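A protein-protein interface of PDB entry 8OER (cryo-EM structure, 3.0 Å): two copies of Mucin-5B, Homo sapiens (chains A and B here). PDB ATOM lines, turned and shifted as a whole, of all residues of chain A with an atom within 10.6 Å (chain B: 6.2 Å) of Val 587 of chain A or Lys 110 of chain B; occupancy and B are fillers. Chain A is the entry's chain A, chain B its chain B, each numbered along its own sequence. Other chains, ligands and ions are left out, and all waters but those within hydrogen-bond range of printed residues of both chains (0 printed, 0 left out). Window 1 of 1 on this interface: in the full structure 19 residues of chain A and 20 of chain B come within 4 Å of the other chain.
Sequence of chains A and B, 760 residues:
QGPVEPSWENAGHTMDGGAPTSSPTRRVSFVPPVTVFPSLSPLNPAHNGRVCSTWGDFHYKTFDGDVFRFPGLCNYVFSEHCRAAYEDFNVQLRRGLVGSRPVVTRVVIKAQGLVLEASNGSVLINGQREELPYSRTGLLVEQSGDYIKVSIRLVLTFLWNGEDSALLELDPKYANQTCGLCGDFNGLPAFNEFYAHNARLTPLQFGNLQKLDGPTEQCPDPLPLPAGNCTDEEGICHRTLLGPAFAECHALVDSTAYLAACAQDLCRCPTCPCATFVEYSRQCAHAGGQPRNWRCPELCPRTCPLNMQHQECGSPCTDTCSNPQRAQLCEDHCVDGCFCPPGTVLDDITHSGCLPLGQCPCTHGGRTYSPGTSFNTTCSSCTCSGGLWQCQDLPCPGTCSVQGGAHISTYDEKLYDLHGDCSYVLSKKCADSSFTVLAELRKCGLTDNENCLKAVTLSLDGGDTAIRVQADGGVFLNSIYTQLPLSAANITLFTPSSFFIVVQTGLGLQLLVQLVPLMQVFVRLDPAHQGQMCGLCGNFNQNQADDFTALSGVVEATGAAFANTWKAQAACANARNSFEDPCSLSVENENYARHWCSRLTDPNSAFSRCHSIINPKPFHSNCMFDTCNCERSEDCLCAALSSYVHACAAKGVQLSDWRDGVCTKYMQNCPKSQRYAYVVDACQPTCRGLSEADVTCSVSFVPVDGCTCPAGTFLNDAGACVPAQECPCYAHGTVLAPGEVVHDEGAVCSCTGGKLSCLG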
ATOM      1  N   ASP A 581      11.375 -24.698  -8.270  1.00  0.00           N
ATOM      2  CA  ASP A 581      11.805 -26.081  -8.355  1.00  0.00           C
ATOM      3  C   ASP A 581      13.104 -26.251  -7.585  1.00  0.00           C
ATOM      4  O   ASP A 581      14.090 -25.580  -7.901  1.00  0.00           O
ATOM      5  CB  ASP A 581      12.006 -26.482  -9.810  1.00  0.00           C
ATOM      6  CG  ASP A 581      12.349 -27.951  -9.973  1.00  0.00           C
ATOM      7  OD1 ASP A 581      12.336 -28.696  -8.974  1.00  0.00           O
ATOM      8  OD2 ASP A 581      12.635 -28.360 -11.117  1.00  0.00           O
ATOM      9  N   PRO A 582      13.156 -27.135  -6.586  1.00  0.00           N
ATOM     10  CA  PRO A 582      14.428 -27.393  -5.899  1.00  0.00           C
ATOM     11  C   PRO A 582      15.478 -27.972  -6.811  1.00  0.00           C
ATOM     12  O   PRO A 582      16.657 -27.993  -6.440  1.00  0.00           O
ATOM     13  CB  PRO A 582      14.036 -28.387  -4.800  1.00  0.00           C
ATOM     14  CG  PRO A 582      12.573 -28.188  -4.619  1.00  0.00           C
ATOM     15  CD  PRO A 582      12.049 -27.885  -5.980  1.00  0.00           C
ATOM     16  N   CYS A 583      15.086 -28.446  -7.990  1.00  0.00           N
ATOM     17  CA  CYS A 583      16.046 -29.016  -8.920  1.00  0.00           C
ATOM     18  C   CYS A 583      17.061 -27.987  -9.398  1.00  0.00           C
ATOM     19  O   CYS A 583      18.194 -28.347  -9.725  1.00  0.00           O
ATOM     20  CB  CYS A 583      15.293 -29.634 -10.094  1.00  0.00           C
ATOM     21  SG  CYS A 583      14.756 -31.341  -9.809  1.00  0.00           S
ATOM     22  N   SER A 584      16.691 -26.711  -9.418  1.00  0.00           N
ATOM     23  CA  SER A 584      17.569 -25.664  -9.926  1.00  0.00           C
ATOM     24  C   SER A 584      18.714 -25.319  -8.981  1.00  0.00           C
ATOM     25  O   SER A 584      19.597 -24.550  -9.366  1.00  0.00           O
ATOM     26  CB  SER A 584      16.758 -24.399 -10.221  1.00  0.00           C
ATOM     27  OG  SER A 584      16.476 -23.683  -9.031  1.00  0.00           O
ATOM     28  N   LEU A 585      18.726 -25.861  -7.764  1.00  0.00           N
ATOM     29  CA  LEU A 585      19.694 -25.420  -6.766  1.00  0.00           C
ATOM     30  C   LEU A 585      21.078 -25.995  -7.026  1.00  0.00           C
ATOM     31  O   LEU A 585      22.032 -25.253  -7.271  1.00  0.00           O
ATOM     32  CB  LEU A 585      19.216 -25.809  -5.369  1.00  0.00           C
ATOM     33  CG  LEU A 585      17.874 -25.222  -4.938  1.00  0.00           C
ATOM     34  CD1 LEU A 585      17.417 -25.858  -3.637  1.00  0.00           C
ATOM     35  CD2 LEU A 585      17.969 -23.712  -4.801  1.00  0.00           C
ATOM     36  N   SER A 586      21.211 -27.313  -6.981  1.00  0.00           N
ATOM     37  CA  SER A 586      22.510 -27.967  -7.031  1.00  0.00           C
ATOM     38  C   SER A 586      22.677 -28.725  -8.337  1.00  0.00           C
ATOM     39  O   SER A 586      21.818 -29.529  -8.708  1.00  0.00           O
ATOM     40  CB  SER A 586      22.683 -28.923  -5.855  1.00  0.00           C
ATOM     41  OG  SER A 586      23.440 -30.054  -6.242  1.00  0.00           O
ATOM     42  N   VAL A 587      23.795 -28.480  -9.020  1.00  0.00           N
ATOM     43  CA  VAL A 587      24.047 -29.148 -10.290  1.00  0.00           C
ATOM     44  C   VAL A 587      24.310 -30.634 -10.079  1.00  0.00           C
ATOM     45  O   VAL A 587      23.936 -31.467 -10.913  1.00  0.00           O
ATOM     46  CB  VAL A 587      25.200 -28.454 -11.038  1.00  0.00           C
ATOM     47  CG1 VAL A 587      24.814 -27.025 -11.373  1.00  0.00           C
ATOM     48  CG2 VAL A 587      26.476 -28.479 -10.218  1.00  0.00           C
ATOM     49  N   GLU A 588      24.972 -30.997  -8.980  1.00  0.00           N
ATOM     50  CA  GLU A 588      25.173 -32.416  -8.710  1.00  0.00           C
ATOM     51  C   GLU A 588      23.857 -33.091  -8.349  1.00  0.00           C
ATOM     52  O   GLU A 588      23.590 -34.215  -8.793  1.00  0.00           O
ATOM     53  CB  GLU A 588      26.217 -32.614  -7.612  1.00  0.00           C
ATOM     54  CG  GLU A 588      26.056 -31.725  -6.398  1.00  0.00           C
ATOM     55  CD  GLU A 588      26.738 -30.386  -6.560  1.00  0.00           C
ATOM     56  OE1 GLU A 588      26.204 -29.541  -7.302  1.00  0.00           O
ATOM     57  OE2 GLU A 588      27.806 -30.178  -5.949  1.00  0.00           O
ATOM     58  N   ASN A 589      23.016 -32.416  -7.557  1.00  0.00           N
ATOM     59  CA  ASN A 589      21.661 -32.909  -7.328  1.00  0.00           C
ATOM     60  C   ASN A 589      20.911 -33.041  -8.645  1.00  0.00           C
ATOM     61  O   ASN A 589      20.208 -34.032  -8.874  1.00  0.00           O
ATOM     62  CB  ASN A 589      20.906 -31.972  -6.384  1.00  0.00           C
ATOM     63  CG  ASN A 589      20.926 -32.443  -4.945  1.00  0.00           C
ATOM     64  OD1 ASN A 589      21.482 -33.491  -4.628  1.00  0.00           O
ATOM     65  ND2 ASN A 589      20.318 -31.664  -4.063  1.00  0.00           N
ATOM     66  N   GLU A 590      21.050 -32.042  -9.516  1.00  0.00           N
ATOM     67  CA  GLU A 590      20.480 -32.118 -10.855  1.00  0.00           C
ATOM     68  C   GLU A 590      20.864 -33.403 -11.557  1.00  0.00           C
ATOM     69  O   GLU A 590      19.997 -34.183 -11.958  1.00  0.00           O
ATOM     70  CB  GLU A 590      20.926 -30.917 -11.682  1.00  0.00           C
ATOM     71  CG  GLU A 590      19.837 -29.933 -11.876  1.00  0.00           C
ATOM     72  CD  GLU A 590      18.520 -30.636 -11.989  1.00  0.00           C
ATOM     73  OE1 GLU A 590      18.230 -31.182 -13.072  1.00  0.00           O
ATOM     74  OE2 GLU A 590      17.801 -30.701 -10.982  1.00  0.00           O
ATOM     75  N   ASN A 591      22.160 -33.622 -11.750  1.00  0.00           N
ATOM     76  CA  ASN A 591      22.586 -34.756 -12.554  1.00  0.00           C
ATOM     77  C   ASN A 591      22.209 -36.072 -11.891  1.00  0.00           C
ATOM     78  O   ASN A 591      21.802 -37.017 -12.574  1.00  0.00           O
ATOM     79  CB  ASN A 591      24.085 -34.672 -12.817  1.00  0.00           C
ATOM     80  CG  ASN A 591      24.422 -33.662 -13.893  1.00  0.00           C
ATOM     81  OD1 ASN A 591      23.968 -32.518 -13.847  1.00  0.00           O
ATOM     82  ND2 ASN A 591      25.209 -34.082 -14.874  1.00  0.00           N
ATOM     83  N   TYR A 592      22.312 -36.147 -10.565  1.00  0.00           N
ATOM     84  CA  TYR A 592      21.930 -37.365  -9.860  1.00  0.00           C
ATOM     85  C   TYR A 592      20.457 -37.685 -10.082  1.00  0.00           C
ATOM     86  O   TYR A 592      20.100 -38.789 -10.524  1.00  0.00           O
ATOM     87  CB  TYR A 592      22.242 -37.194  -8.374  1.00  0.00           C
ATOM     88  CG  TYR A 592      21.814 -38.331  -7.483  1.00  0.00           C
ATOM     89  CD1 TYR A 592      22.654 -39.406  -7.245  1.00  0.00           C
ATOM     90  CD2 TYR A 592      20.582 -38.312  -6.854  1.00  0.00           C
ATOM     91  CE1 TYR A 592      22.272 -40.435  -6.422  1.00  0.00           C
ATOM     92  CE2 TYR A 592      20.190 -39.337  -6.033  1.00  0.00           C
ATOM     93  CZ  TYR A 592      21.035 -40.396  -5.819  1.00  0.00           C
ATOM     94  OH  TYR A 592      20.639 -41.419  -4.993  1.00  0.00           O
ATOM     95  N   ALA A 593      19.587 -36.709  -9.810  1.00  0.00           N
ATOM     96  CA  ALA A 593      18.154 -36.925  -9.953  1.00  0.00           C
ATOM     97  C   ALA A 593      17.788 -37.236 -11.393  1.00  0.00           C
ATOM     98  O   ALA A 593      16.963 -38.113 -11.650  1.00  0.00           O
ATOM     99  CB  ALA A 593      17.389 -35.699  -9.462  1.00  0.00           C
ATOM    100  N   ARG A 594      18.387 -36.527 -12.347  1.00  0.00           N
ATOM    101  CA  ARG A 594      18.086 -36.788 -13.747  1.00  0.00           C
ATOM    102  C   ARG A 594      18.494 -38.198 -14.134  1.00  0.00           C
ATOM    103  O   ARG A 594      17.674 -38.980 -14.626  1.00  0.00           O
ATOM    104  CB  ARG A 594      18.794 -35.764 -14.629  1.00  0.00           C
ATOM    105  CG  ARG A 594      18.776 -36.102 -16.100  1.00  0.00           C
ATOM    106  CD  ARG A 594      19.701 -35.186 -16.872  1.00  0.00           C
ATOM    107  NE  ARG A 594      19.353 -33.783 -16.681  1.00  0.00           N
ATOM    108  CZ  ARG A 594      20.134 -32.895 -16.085  1.00  0.00           C
ATOM    109  NH1 ARG A 594      21.324 -33.227 -15.613  1.00  0.00           N
ATOM    110  NH2 ARG A 594      19.710 -31.641 -15.959  1.00  0.00           N
ATOM    111  N   HIS A 595      19.749 -38.560 -13.866  1.00  0.00           N
ATOM    112  CA  HIS A 595      20.250 -39.854 -14.299  1.00  0.00           C
ATOM    113  C   HIS A 595      19.501 -40.998 -13.635  1.00  0.00           C
ATOM    114  O   HIS A 595      19.428 -42.095 -14.201  1.00  0.00           O
ATOM    115  CB  HIS A 595      21.747 -39.957 -14.016  1.00  0.00           C
ATOM    116  CG  HIS A 595      22.249 -41.364 -13.943  1.00  0.00           C
ATOM    117  ND1 HIS A 595      22.000 -42.292 -14.931  1.00  0.00           N
ATOM    118  CD2 HIS A 595      22.978 -42.004 -13.000  1.00  0.00           C
ATOM    119  CE1 HIS A 595      22.554 -43.444 -14.598  1.00  0.00           C
ATOM    120  NE2 HIS A 595      23.154 -43.296 -13.432  1.00  0.00           N
ATOM    121  N   MET A 624      11.685 -36.289  -9.783  1.00  0.00           N
ATOM    122  CA  MET A 624      12.545 -35.117  -9.887  1.00  0.00           C
ATOM    123  C   MET A 624      12.423 -34.235  -8.655  1.00  0.00           C
ATOM    124  O   MET A 624      13.425 -33.907  -8.006  1.00  0.00           O
ATOM    125  CB  MET A 624      12.176 -34.317 -11.134  1.00  0.00           C
ATOM    126  CG  MET A 624      13.331 -33.882 -12.007  1.00  0.00           C
ATOM    127  SD  MET A 624      14.393 -35.202 -12.592  1.00  0.00           S
ATOM    128  CE  MET A 624      15.730 -34.223 -13.264  1.00  0.00           C
ATOM    129  N   THR A 627      13.749 -36.044  -5.310  1.00  0.00           N
ATOM    130  CA  THR A 627      15.193 -36.232  -5.228  1.00  0.00           C
ATOM    131  C   THR A 627      15.925 -34.904  -5.128  1.00  0.00           C
ATOM    132  O   THR A 627      16.874 -34.771  -4.349  1.00  0.00           O
ATOM    133  CB  THR A 627      15.689 -37.015  -6.432  1.00  0.00           C
ATOM    134  OG1 THR A 627      14.924 -38.218  -6.562  1.00  0.00           O
ATOM    135  CG2 THR A 627      17.148 -37.367  -6.249  1.00  0.00           C
ATOM    136  N   CYS A 628      15.497 -33.904  -5.898  1.00  0.00           N
ATOM    137  CA  CYS A 628      16.140 -32.600  -5.808  1.00  0.00           C
ATOM    138  C   CYS A 628      15.914 -31.964  -4.445  1.00  0.00           C
ATOM    139  O   CYS A 628      16.831 -31.366  -3.873  1.00  0.00           O
ATOM    140  CB  CYS A 628      15.621 -31.692  -6.916  1.00  0.00           C
ATOM    141  SG  CYS A 628      16.164 -32.140  -8.581  1.00  0.00           S
ATOM    142  N   SER A 633      18.471 -38.117  -0.806  1.00  0.00           N
ATOM    143  CA  SER A 633      18.057 -38.199  -2.201  1.00  0.00           C
ATOM    144  C   SER A 633      17.691 -39.620  -2.588  1.00  0.00           C
ATOM    145  O   SER A 633      16.698 -39.845  -3.289  1.00  0.00           O
ATOM    146  CB  SER A 633      19.168 -37.671  -3.103  1.00  0.00           C
ATOM    147  OG  SER A 633      19.464 -36.321  -2.802  1.00  0.00           O
ATOM    148  N   GLU B  87      16.219 -17.076 -10.892  1.00  0.00           N
ATOM    149  CA  GLU B  87      17.557 -16.880 -10.354  1.00  0.00           C
ATOM    150  C   GLU B  87      18.525 -16.463 -11.453  1.00  0.00           C
ATOM    151  O   GLU B  87      18.413 -16.883 -12.607  1.00  0.00           O
ATOM    152  CB  GLU B  87      18.063 -18.152  -9.670  1.00  0.00           C
ATOM    153  CG  GLU B  87      18.781 -19.137 -10.586  1.00  0.00           C
ATOM    154  CD  GLU B  87      19.321 -20.341  -9.839  1.00  0.00           C
ATOM    155  OE1 GLU B  87      19.267 -20.342  -8.593  1.00  0.00           O
ATOM    156  OE2 GLU B  87      19.798 -21.288 -10.495  1.00  0.00           O
ATOM    157  N   ASP B  88      19.478 -15.612 -11.082  1.00  0.00           N
ATOM    158  CA  ASP B  88      20.499 -15.140 -12.007  1.00  0.00           C
ATOM    159  C   ASP B  88      21.866 -15.747 -11.746  1.00  0.00           C
ATOM    160  O   ASP B  88      22.597 -16.031 -12.698  1.00  0.00           O
ATOM    161  CB  ASP B  88      20.605 -13.615 -11.935  1.00  0.00           C
ATOM    162  CG  ASP B  88      19.494 -12.923 -12.684  1.00  0.00           C
ATOM    163  OD1 ASP B  88      18.884 -13.567 -13.558  1.00  0.00           O
ATOM    164  OD2 ASP B  88      19.224 -11.740 -12.399  1.00  0.00           O
ATOM    165  N   PHE B  89      22.225 -15.955 -10.484  1.00  0.00           N
ATOM    166  CA  PHE B  89      23.524 -16.502 -10.136  1.00  0.00           C
ATOM    167  C   PHE B  89      23.376 -17.410  -8.928  1.00  0.00           C
ATOM    168  O   PHE B  89      22.485 -17.222  -8.097  1.00  0.00           O
ATOM    169  CB  PHE B  89      24.541 -15.404  -9.821  1.00  0.00           C
ATOM    170  CG  PHE B  89      24.080 -14.437  -8.783  1.00  0.00           C
ATOM    171  CD1 PHE B  89      23.214 -13.417  -9.102  1.00  0.00           C
ATOM    172  CD2 PHE B  89      24.491 -14.566  -7.477  1.00  0.00           C
ATOM    173  CE1 PHE B  89      22.786 -12.536  -8.145  1.00  0.00           C
ATOM    174  CE2 PHE B  89      24.058 -13.683  -6.514  1.00  0.00           C
ATOM    175  CZ  PHE B  89      23.205 -12.669  -6.852  1.00  0.00           C
ATOM    176  N   ASN B  90      24.270 -18.390  -8.834  1.00  0.00           N
ATOM    177  CA  ASN B  90      24.287 -19.320  -7.706  1.00  0.00           C
ATOM    178  C   ASN B  90      25.743 -19.738  -7.501  1.00  0.00           C
ATOM    179  O   ASN B  90      26.227 -20.670  -8.144  1.00  0.00           O
ATOM    180  CB  ASN B  90      23.385 -20.515  -7.966  1.00  0.00           C
ATOM    181  CG  ASN B  90      23.384 -21.509  -6.833  1.00  0.00           C
ATOM    182  OD1 ASN B  90      24.375 -22.188  -6.584  1.00  0.00           O
ATOM    183  ND2 ASN B  90      22.262 -21.605  -6.137  1.00  0.00           N
ATOM    184  N   VAL B  91      26.430 -19.040  -6.601  1.00  0.00           N
ATOM    185  CA  VAL B  91      27.839 -19.272  -6.322  1.00  0.00           C
ATOM    186  C   VAL B  91      27.957 -19.961  -4.971  1.00  0.00           C
ATOM    187  O   VAL B  91      27.400 -19.487  -3.974  1.00  0.00           O
ATOM    188  CB  VAL B  91      28.637 -17.959  -6.361  1.00  0.00           C
ATOM    189  CG1 VAL B  91      27.830 -16.849  -5.761  1.00  0.00           C
ATOM    190  CG2 VAL B  91      29.937 -18.108  -5.612  1.00  0.00           C
ATOM    191  N   GLN B  92      28.674 -21.084  -4.947  1.00  0.00           N
ATOM    192  CA  GLN B  92      28.838 -21.910  -3.762  1.00  0.00           C
ATOM    193  C   GLN B  92      30.310 -22.228  -3.557  1.00  0.00           C
ATOM    194  O   GLN B  92      31.076 -22.305  -4.519  1.00  0.00           O
ATOM    195  CB  GLN B  92      28.054 -23.212  -3.886  1.00  0.00           C
ATOM    196  CG  GLN B  92      26.595 -23.011  -4.221  1.00  0.00           C
ATOM    197  CD  GLN B  92      25.926 -24.271  -4.716  1.00  0.00           C
ATOM    198  OE1 GLN B  92      26.457 -25.368  -4.574  1.00  0.00           O
ATOM    199  NE2 GLN B  92      24.749 -24.118  -5.304  1.00  0.00           N
ATOM    200  N   ARG B 106      36.743 -26.157  -3.889  1.00  0.00           N
ATOM    201  CA  ARG B 106      35.938 -26.152  -5.103  1.00  0.00           C
ATOM    202  C   ARG B 106      34.905 -25.044  -5.014  1.00  0.00           C
ATOM    203  O   ARG B 106      34.270 -24.870  -3.972  1.00  0.00           O
ATOM    204  CB  ARG B 106      35.262 -27.512  -5.313  1.00  0.00           C
ATOM    205  CG  ARG B 106      34.183 -27.546  -6.375  1.00  0.00           C
ATOM    206  CD  ARG B 106      33.284 -28.755  -6.183  1.00  0.00           C
ATOM    207  NE  ARG B 106      32.231 -28.525  -5.203  1.00  0.00           N
ATOM    208  CZ  ARG B 106      30.945 -28.766  -5.417  1.00  0.00           C
ATOM    209  NH1 ARG B 106      30.519 -29.265  -6.566  1.00  0.00           N
ATOM    210  NH2 ARG B 106      30.068 -28.507  -4.453  1.00  0.00           N
ATOM    211  N   VAL B 108      31.534 -23.504  -7.250  1.00  0.00           N
ATOM    212  CA  VAL B 108      30.587 -23.765  -8.326  1.00  0.00           C
ATOM    213  C   VAL B 108      29.755 -22.510  -8.515  1.00  0.00           C
ATOM    214  O   VAL B 108      28.967 -22.141  -7.636  1.00  0.00           O
ATOM    215  CB  VAL B 108      29.696 -24.974  -8.036  1.00  0.00           C
ATOM    216  CG1 VAL B 108      28.635 -25.098  -9.098  1.00  0.00           C
ATOM    217  CG2 VAL B 108      30.529 -26.228  -7.982  1.00  0.00           C
ATOM    218  N   ILE B 109      29.927 -21.854  -9.655  1.00  0.00           N
ATOM    219  CA  ILE B 109      29.145 -20.684 -10.018  1.00  0.00           C
ATOM    220  C   ILE B 109      28.184 -21.100 -11.115  1.00  0.00           C
ATOM    221  O   ILE B 109      28.606 -21.443 -12.223  1.00  0.00           O
ATOM    222  CB  ILE B 109      30.038 -19.530 -10.487  1.00  0.00           C
ATOM    223  CG1 ILE B 109      31.075 -19.192  -9.427  1.00  0.00           C
ATOM    224  CG2 ILE B 109      29.199 -18.314 -10.782  1.00  0.00           C
ATOM    225  CD1 ILE B 109      32.059 -18.167  -9.875  1.00  0.00           C
ATOM    226  N   LYS B 110      26.899 -21.081 -10.810  1.00  0.00           N
ATOM    227  CA  LYS B 110      25.860 -21.322 -11.797  1.00  0.00           C
ATOM    228  C   LYS B 110      25.222 -19.982 -12.115  1.00  0.00           C
ATOM    229  O   LYS B 110      24.821 -19.253 -11.200  1.00  0.00           O
ATOM    230  CB  LYS B 110      24.825 -22.310 -11.271  1.00  0.00           C
ATOM    231  CG  LYS B 110      23.752 -22.664 -12.268  1.00  0.00           C
ATOM    232  CD  LYS B 110      22.788 -23.671 -11.682  1.00  0.00           C
ATOM    233  CE  LYS B 110      21.686 -24.011 -12.662  1.00  0.00           C
ATOM    234  NZ  LYS B 110      20.743 -25.016 -12.103  1.00  0.00           N
ATOM    235  N   ALA B 111      25.139 -19.649 -13.397  1.00  0.00           N
ATOM    236  CA  ALA B 111      24.612 -18.347 -13.783  1.00  0.00           C
ATOM    237  C   ALA B 111      24.061 -18.424 -15.193  1.00  0.00           C
ATOM    238  O   ALA B 111      24.811 -18.673 -16.139  1.00  0.00           O
ATOM    239  CB  ALA B 111      25.689 -17.269 -13.689  1.00  0.00           C
ATOM    240  N   GLN B 112      22.754 -18.214 -15.319  1.00  0.00           N
ATOM    241  CA  GLN B 112      22.120 -17.972 -16.607  1.00  0.00           C
ATOM    242  C   GLN B 112      22.384 -19.120 -17.574  1.00  0.00           C
ATOM    243  O   GLN B 112      22.642 -18.916 -18.760  1.00  0.00           O
ATOM    244  CB  GLN B 112      22.602 -16.642 -17.189  1.00  0.00           C
ATOM    245  CG  GLN B 112      22.189 -15.389 -16.401  1.00  0.00           C
ATOM    246  CD  GLN B 112      20.693 -15.138 -16.331  1.00  0.00           C
ATOM    247  OE1 GLN B 112      19.884 -16.060 -16.254  1.00  0.00           O
ATOM    248  NE2 GLN B 112      20.320 -13.867 -16.331  1.00  0.00           N
ATOM    249  N   GLY B 113      22.329 -20.343 -17.057  1.00  0.00           N
ATOM    250  CA  GLY B 113      22.537 -21.513 -17.884  1.00  0.00           C
ATOM    251  C   GLY B 113      23.979 -21.882 -18.135  1.00  0.00           C
ATOM    252  O   GLY B 113      24.247 -22.725 -18.997  1.00  0.00           O
ATOM    253  N   LEU B 114      24.915 -21.277 -17.419  1.00  0.00           N
ATOM    254  CA  LEU B 114      26.325 -21.608 -17.525  1.00  0.00           C
ATOM    255  C   LEU B 114      26.824 -22.103 -16.177  1.00  0.00           C
ATOM    256  O   LEU B 114      26.606 -21.448 -15.154  1.00  0.00           O
ATOM    257  CB  LEU B 114      27.122 -20.393 -17.986  1.00  0.00           C
ATOM    258  CG  LEU B 114      28.631 -20.462 -17.820  1.00  0.00           C
ATOM    259  CD1 LEU B 114      29.270 -19.894 -19.062  1.00  0.00           C
ATOM    260  CD2 LEU B 114      29.048 -19.681 -16.588  1.00  0.00           C
ATOM    261  N   VAL B 115      27.495 -23.252 -16.179  1.00  0.00           N
ATOM    262  CA  VAL B 115      27.990 -23.886 -14.964  1.00  0.00           C
ATOM    263  C   VAL B 115      29.509 -23.834 -14.980  1.00  0.00           C
ATOM    264  O   VAL B 115      30.140 -24.349 -15.909  1.00  0.00           O
ATOM    265  CB  VAL B 115      27.500 -25.336 -14.849  1.00  0.00           C
ATOM    266  CG1 VAL B 115      27.998 -25.957 -13.564  1.00  0.00           C
ATOM    267  CG2 VAL B 115      25.995 -25.384 -14.931  1.00  0.00           C
ATOM    268  N   LEU B 116      30.097 -23.235 -13.949  1.00  0.00           N
ATOM    269  CA  LEU B 116      31.536 -23.010 -13.897  1.00  0.00           C
ATOM    270  C   LEU B 116      32.056 -23.564 -12.584  1.00  0.00           C
ATOM    271  O   LEU B 116      31.757 -23.023 -11.518  1.00  0.00           O
ATOM    272  CB  LEU B 116      31.847 -21.525 -14.034  1.00  0.00           C
ATOM    273  CG  LEU B 116      33.286 -21.024 -14.065  1.00  0.00           C
ATOM    274  CD1 LEU B 116      33.240 -19.643 -14.641  1.00  0.00           C
ATOM    275  CD2 LEU B 116      33.959 -20.984 -12.701  1.00  0.00           C
ATOM    276  N   GLU B 117      32.846 -24.625 -12.657  1.00  0.00           N
ATOM    277  CA  GLU B 117      33.343 -25.313 -11.472  1.00  0.00           C
ATOM    278  C   GLU B 117      34.859 -25.186 -11.433  1.00  0.00           C
ATOM    279  O   GLU B 117      35.558 -25.764 -12.268  1.00  0.00           O
ATOM    280  CB  GLU B 117      32.902 -26.773 -11.474  1.00  0.00           C
ATOM    281  CG  GLU B 117      33.316 -27.538 -10.240  1.00  0.00           C
ATOM    282  CD  GLU B 117      32.888 -28.988 -10.289  1.00  0.00           C
ATOM    283  OE1 GLU B 117      32.277 -29.392 -11.300  1.00  0.00           O
ATOM    284  OE2 GLU B 117      33.165 -29.725  -9.318  1.00  0.00           O
ATOM    285  N   LEU B 156      28.346 -10.343 -12.055  1.00  0.00           N
ATOM    286  CA  LEU B 156      29.201 -10.520 -10.896  1.00  0.00           C
ATOM    287  C   LEU B 156      30.666 -10.532 -11.297  1.00  0.00           C
ATOM    288  O   LEU B 156      31.022 -10.642 -12.474  1.00  0.00           O
ATOM    289  CB  LEU B 156      28.834 -11.804 -10.139  1.00  0.00           C
ATOM    290  CG  LEU B 156      28.896 -13.160 -10.842  1.00  0.00           C
ATOM    291  CD1 LEU B 156      30.290 -13.737 -10.857  1.00  0.00           C
ATOM    292  CD2 LEU B 156      27.959 -14.120 -10.168  1.00  0.00           C
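The backbone carbonyl oxygen of Ser 584 of chain A is in hydrogen-bond range of the side-chain amino group of Lys 110 of chain B (3.0 Å).
OE2 of Glu 588 of chain A is in salt-bridge range of NH1 of Arg 106 of chain B, 2.9 Å away.
The backbone carbonyl oxygen (O) of Ser 584 of chain A sits close to the side-chain carboxylate (OE2) of Glu 87 of chain B, at 3.5 Å.
The side-chain carboxylate (OE2) of Glu 117 of chain B lies within salt-bridge range of the guanidinium group (NH1) of Arg 106 of chain B, 3.8 Å away.
O of Val 108 of chain B lies within hydrogen-bond range of N of Gln 92 of chain B.
OG of Ser 586 of chain A lies within hydrogen-bond range of OE1 of Glu 588 of chain A.
The backbone carbonyl oxygen (O) of Asp 581 of chain A is in hydrogen-bond range of the side-chain hydroxyl (OG) of Ser 584 of chain A (3.3 Å).
The side-chain amide oxygen of Asn 591 of chain A sits close to the backbone carbonyl oxygen of Val 587 of chain A (3.1 Å).
Among the printed residues, pairs that only touch across the chains: Leu 585 of chain A with Gln 92 of chain B, Leu 585 of chain A with Asn 90 of chain B and Val 587 of chain A with Lys 110 of chain B.
Printed residues of chain B within 4 Å of Ser 584 of chain A: Glu 87 and Lys 110.
Printed residues of chain B within 4 Å of Leu 585 of chain A: Asn 90 (3.8 Å) and Gln 92 (3.5 Å).
Printed residues of chain B within 4 Å of Val 587 of chain A: Lys 110.
Of the printed residues of chain B, Glu 588 of chain A touches Arg 106.
Asp 88 of chain B touches none of the printed residues of chain A.
No residue of chain A comes within 4 Å of Ile 109 of chain B.
Lys 110 of chain B touches two residues of chain A.
Glu 117 of chain B touches none of the printed residues of chain A.
The nearest residue of chain A that does not touch Lys 110 of chain B is Leu 585 of chain A (4.7 Å).
The nearest printed residue of chain B that does not touch Glu 588 of chain A is Gln 92 of chain B (5.0 Å).
Of the 19 printed residues of chain A, 4 touch a printed residue of chain B.
Printed residues of chain A that touch a printed residue of chain B: Ser 584, Leu 585, Val 587 and Glu 588.
Hydrophobic or aromatic side chains of chain A within 4 Å of the printed part of chain B: Val 587.
Along chain A the printed residues that touch a printed residue of chain B span positions 584 to 588.
Of the 18 printed residues of chain B, 5 touch a printed residue of chain A.
Printed residues of chain B that touch a printed residue of chain A: Glu 87, Asn 90, Gln 92, Arg 106 and Lys 110.
Among the printed residues, Asp or Glu carboxylates within 4 Å of a Lys or Arg side-chain nitrogen of the other chain: Glu 588 of chain A with Arg 106 of chain B (2.9 Å).
No position is printed for both chains.
Of the 6 pairs that touch across the chains among the printed residues, none has its exchanged pair printed and touching as well.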
